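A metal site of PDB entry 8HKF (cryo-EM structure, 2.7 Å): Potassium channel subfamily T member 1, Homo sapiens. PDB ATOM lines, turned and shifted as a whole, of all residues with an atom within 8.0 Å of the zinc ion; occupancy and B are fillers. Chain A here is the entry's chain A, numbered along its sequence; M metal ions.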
ATOM      1  N   ALA A 774     -23.776  -6.926   4.360  1.00  0.00           N
ATOM      2  CA  ALA A 774     -24.031  -7.338   5.729  1.00  0.00           C
ATOM      3  C   ALA A 774     -23.254  -6.433   6.689  1.00  0.00           C
ATOM      4  O   ALA A 774     -22.045  -6.248   6.514  1.00  0.00           O
ATOM      5  CB  ALA A 774     -23.623  -8.790   5.937  1.00  0.00           C
ATOM      6  N   PRO A 775     -23.917  -5.849   7.686  1.00  0.00           N
ATOM      7  CA  PRO A 775     -23.180  -5.081   8.696  1.00  0.00           C
ATOM      8  C   PRO A 775     -22.198  -5.969   9.449  1.00  0.00           C
ATOM      9  O   PRO A 775     -22.416  -7.168   9.603  1.00  0.00           O
ATOM     10  CB  PRO A 775     -24.279  -4.554   9.620  1.00  0.00           C
ATOM     11  CG  PRO A 775     -25.497  -5.368   9.302  1.00  0.00           C
ATOM     12  CD  PRO A 775     -25.367  -5.752   7.872  1.00  0.00           C
ATOM     13  N   PHE A 776     -21.099  -5.364   9.899  1.00  0.00           N
ATOM     14  CA  PHE A 776     -20.034  -6.109  10.546  1.00  0.00           C
ATOM     15  C   PHE A 776     -20.515  -6.832  11.800  1.00  0.00           C
ATOM     16  O   PHE A 776     -19.880  -7.801  12.220  1.00  0.00           O
ATOM     17  CB  PHE A 776     -18.865  -5.187  10.903  1.00  0.00           C
ATOM     18  CG  PHE A 776     -18.113  -4.663   9.709  1.00  0.00           C
ATOM     19  CD1 PHE A 776     -18.531  -4.934   8.421  1.00  0.00           C
ATOM     20  CD2 PHE A 776     -16.991  -3.876   9.884  1.00  0.00           C
ATOM     21  CE1 PHE A 776     -17.841  -4.438   7.329  1.00  0.00           C
ATOM     22  CE2 PHE A 776     -16.296  -3.379   8.805  1.00  0.00           C
ATOM     23  CZ  PHE A 776     -16.719  -3.662   7.519  1.00  0.00           C
ATOM     24  N   CYS A 777     -21.619  -6.377  12.392  1.00  0.00           N
ATOM     25  CA  CYS A 777     -22.186  -7.060  13.538  1.00  0.00           C
ATOM     26  C   CYS A 777     -22.829  -8.393  13.136  1.00  0.00           C
ATOM     27  O   CYS A 777     -22.845  -9.334  13.940  1.00  0.00           O
ATOM     28  CB  CYS A 777     -23.217  -6.171  14.229  1.00  0.00           C
ATOM     29  SG  CYS A 777     -24.644  -5.768  13.210  1.00  0.00           S
ATOM     30  N   CYS A 778     -23.370  -8.469  11.921  1.00  0.00           N
ATOM     31  CA  CYS A 778     -24.028  -9.688  11.476  1.00  0.00           C
ATOM     32  C   CYS A 778     -23.048 -10.730  10.969  1.00  0.00           C
ATOM     33  O   CYS A 778     -23.462 -11.858  10.667  1.00  0.00           O
ATOM     34  CB  CYS A 778     -25.058  -9.362  10.399  1.00  0.00           C
ATOM     35  SG  CYS A 778     -26.443  -8.362  10.977  1.00  0.00           S
ATOM     36  N   LEU A 779     -21.768 -10.400  10.862  1.00  0.00           N
ATOM     37  CA  LEU A 779     -20.742 -11.350  10.459  1.00  0.00           C
ATOM     38  C   LEU A 779     -20.161 -12.114  11.645  1.00  0.00           C
ATOM     39  O   LEU A 779     -19.323 -13.002  11.428  1.00  0.00           O
ATOM     40  CB  LEU A 779     -19.615 -10.644   9.707  1.00  0.00           C
ATOM     41  CG  LEU A 779     -20.010  -9.779   8.510  1.00  0.00           C
ATOM     42  CD1 LEU A 779     -18.780  -9.127   7.906  1.00  0.00           C
ATOM     43  CD2 LEU A 779     -20.747 -10.607   7.482  1.00  0.00           C
ATOM     44  N   ARG A 780     -20.571 -11.800  12.861  1.00  0.00           N
ATOM     45  CA  ARG A 780     -19.996 -12.401  14.065  1.00  0.00           C
ATOM     46  C   ARG A 780     -20.928 -13.490  14.575  1.00  0.00           C
ATOM     47  O   ARG A 780     -22.115 -13.247  14.807  1.00  0.00           O
ATOM     48  CB  ARG A 780     -19.758 -11.346  15.145  1.00  0.00           C
ATOM     49  CG  ARG A 780     -18.976 -11.865  16.324  1.00  0.00           C
ATOM     50  CD  ARG A 780     -18.211 -10.750  17.004  1.00  0.00           C
ATOM     51  NE  ARG A 780     -17.321 -11.263  18.044  1.00  0.00           N
ATOM     52  CZ  ARG A 780     -17.349 -10.892  19.309  1.00  0.00           C
ATOM     53  NH1 ARG A 780     -18.216  -9.993  19.740  1.00  0.00           N
ATOM     54  NH2 ARG A 780     -16.478 -11.418  20.168  1.00  0.00           N
ATOM     55  N   LYS A 783     -21.386 -13.009  19.249  1.00  0.00           N
ATOM     56  CA  LYS A 783     -22.270 -12.045  19.885  1.00  0.00           C
ATOM     57  C   LYS A 783     -23.546 -11.879  19.082  1.00  0.00           C
ATOM     58  O   LYS A 783     -23.547 -11.979  17.849  1.00  0.00           O
ATOM     59  CB  LYS A 783     -21.575 -10.695  20.032  1.00  0.00           C
ATOM     60  CG  LYS A 783     -21.164 -10.051  18.720  1.00  0.00           C
ATOM     61  CD  LYS A 783     -21.525  -8.582  18.659  1.00  0.00           C
ATOM     62  CE  LYS A 783     -21.332  -8.023  17.270  1.00  0.00           C
ATOM     63  NZ  LYS A 783     -22.226  -8.675  16.278  1.00  0.00           N
ATOM     64  N   GLY A 784     -24.645 -11.656  19.791  1.00  0.00           N
ATOM     65  CA  GLY A 784     -25.872 -11.237  19.144  1.00  0.00           C
ATOM     66  C   GLY A 784     -25.866  -9.747  18.860  1.00  0.00           C
ATOM     67  O   GLY A 784     -25.183  -8.966  19.511  1.00  0.00           O
ATOM     68  N   CYS A 785     -26.651  -9.354  17.860  1.00  0.00           N
ATOM     69  CA  CYS A 785     -26.744  -7.955  17.486  1.00  0.00           C
ATOM     70  C   CYS A 785     -28.188  -7.527  17.366  1.00  0.00           C
ATOM     71  O   CYS A 785     -29.100  -8.244  17.796  1.00  0.00           O
ATOM     72  CB  CYS A 785     -25.981  -7.690  16.184  1.00  0.00           C
ATOM     73  SG  CYS A 785     -26.457  -8.739  14.798  1.00  0.00           S
ATOM     74  N   LYS A 786     -28.423  -6.354  16.793  1.00  0.00           N
ATOM     75  CA  LYS A 786     -29.772  -5.831  16.644  1.00  0.00           C
ATOM     76  C   LYS A 786     -30.596  -6.738  15.755  1.00  0.00           C
ATOM     77  O   LYS A 786     -31.768  -7.008  16.029  1.00  0.00           O
ATOM     78  CB  LYS A 786     -29.752  -4.409  16.081  1.00  0.00           C
ATOM     79  CG  LYS A 786     -29.028  -3.299  16.891  1.00  0.00           C
ATOM     80  CD  LYS A 786     -29.651  -2.995  18.255  1.00  0.00           C
ATOM     81  CE  LYS A 786     -28.915  -1.850  18.943  1.00  0.00           C
ATOM     82  NZ  LYS A 786     -29.489  -1.554  20.290  1.00  0.00           N
ATOM     83  N   HIS A 787     -29.988  -7.235  14.671  1.00  0.00           N
ATOM     84  CA  HIS A 787     -30.725  -8.020  13.685  1.00  0.00           C
ATOM     85  C   HIS A 787     -30.991  -9.446  14.143  1.00  0.00           C
ATOM     86  O   HIS A 787     -32.011 -10.028  13.760  1.00  0.00           O
ATOM     87  CB  HIS A 787     -29.968  -8.004  12.355  1.00  0.00           C
ATOM     88  CG  HIS A 787     -29.338  -6.687  12.036  1.00  0.00           C
ATOM     89  ND1 HIS A 787     -28.182  -6.244  12.654  1.00  0.00           N
ATOM     90  CD2 HIS A 787     -29.710  -5.699  11.182  1.00  0.00           C
ATOM     91  CE1 HIS A 787     -27.866  -5.057  12.176  1.00  0.00           C
ATOM     92  NE2 HIS A 787     -28.772  -4.697  11.285  1.00  0.00           N
ATOM     93  N   ASN A 788     -30.099 -10.034  14.947  1.00  0.00           N
ATOM     94  CA  ASN A 788     -30.336 -11.382  15.447  1.00  0.00           C
ATOM     95  C   ASN A 788     -29.761 -11.544  16.838  1.00  0.00           C
ATOM     96  O   ASN A 788     -28.772 -10.892  17.197  1.00  0.00           O
ATOM     97  CB  ASN A 788     -29.773 -12.450  14.486  1.00  0.00           C
ATOM     98  CG  ASN A 788     -28.344 -12.156  14.038  1.00  0.00           C
ATOM     99  OD1 ASN A 788     -27.431 -12.004  14.849  1.00  0.00           O
ATOM    100  ND2 ASN A 788     -28.147 -12.084  12.722  1.00  0.00           N
ATOM    101  N   SER A 789     -30.390 -12.404  17.638  1.00  0.00           N
ATOM    102  CA  SER A 789     -29.927 -12.736  18.981  1.00  0.00           C
ATOM    103  C   SER A 789     -29.109 -14.017  19.012  1.00  0.00           C
ATOM    104  O   SER A 789     -28.734 -14.476  20.103  1.00  0.00           O
ATOM    105  CB  SER A 789     -31.120 -12.862  19.931  1.00  0.00           C
ATOM    106  OG  SER A 789     -31.963 -13.939  19.558  1.00  0.00           O
ATOM    107  N   TYR A 796     -28.613 -20.345  14.671  1.00  0.00           N
ATOM    108  CA  TYR A 796     -28.818 -19.958  13.288  1.00  0.00           C
ATOM    109  C   TYR A 796     -29.684 -20.958  12.552  1.00  0.00           C
ATOM    110  O   TYR A 796     -30.568 -20.575  11.764  1.00  0.00           O
ATOM    111  CB  TYR A 796     -27.473 -19.803  12.580  1.00  0.00           C
ATOM    112  CG  TYR A 796     -26.769 -18.496  12.856  1.00  0.00           C
ATOM    113  CD1 TYR A 796     -26.071 -18.291  14.031  1.00  0.00           C
ATOM    114  CD2 TYR A 796     -26.829 -17.449  11.941  1.00  0.00           C
ATOM    115  CE1 TYR A 796     -25.429 -17.096  14.287  1.00  0.00           C
ATOM    116  CE2 TYR A 796     -26.192 -16.255  12.184  1.00  0.00           C
ATOM    117  CZ  TYR A 796     -25.497 -16.080  13.363  1.00  0.00           C
ATOM    118  OH  TYR A 796     -24.868 -14.882  13.609  1.00  0.00           O
HETATM  119 ZN    ZN M   1     -26.413  -7.264  13.025  1.00  0.00          ZN
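O of Cys 777 is in hydrogen-bond range of NZ of Lys 783. The side-chain sulfur of Cys 785 sits close to the side-chain amide oxygen of Asn 788 (3.4 Å).
Of the 15 residues printed, 4 come within 4 Å of the zinc ion.
The zinc ion is bound by ND1 of His 787 (2.1 Å), SG of Cys 785 (2.3 Å), SG of Cys 777 (2.3 Å) and SG of Cys 778 (2.3 Å). The zinc ion has four donor atoms within binding distance.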
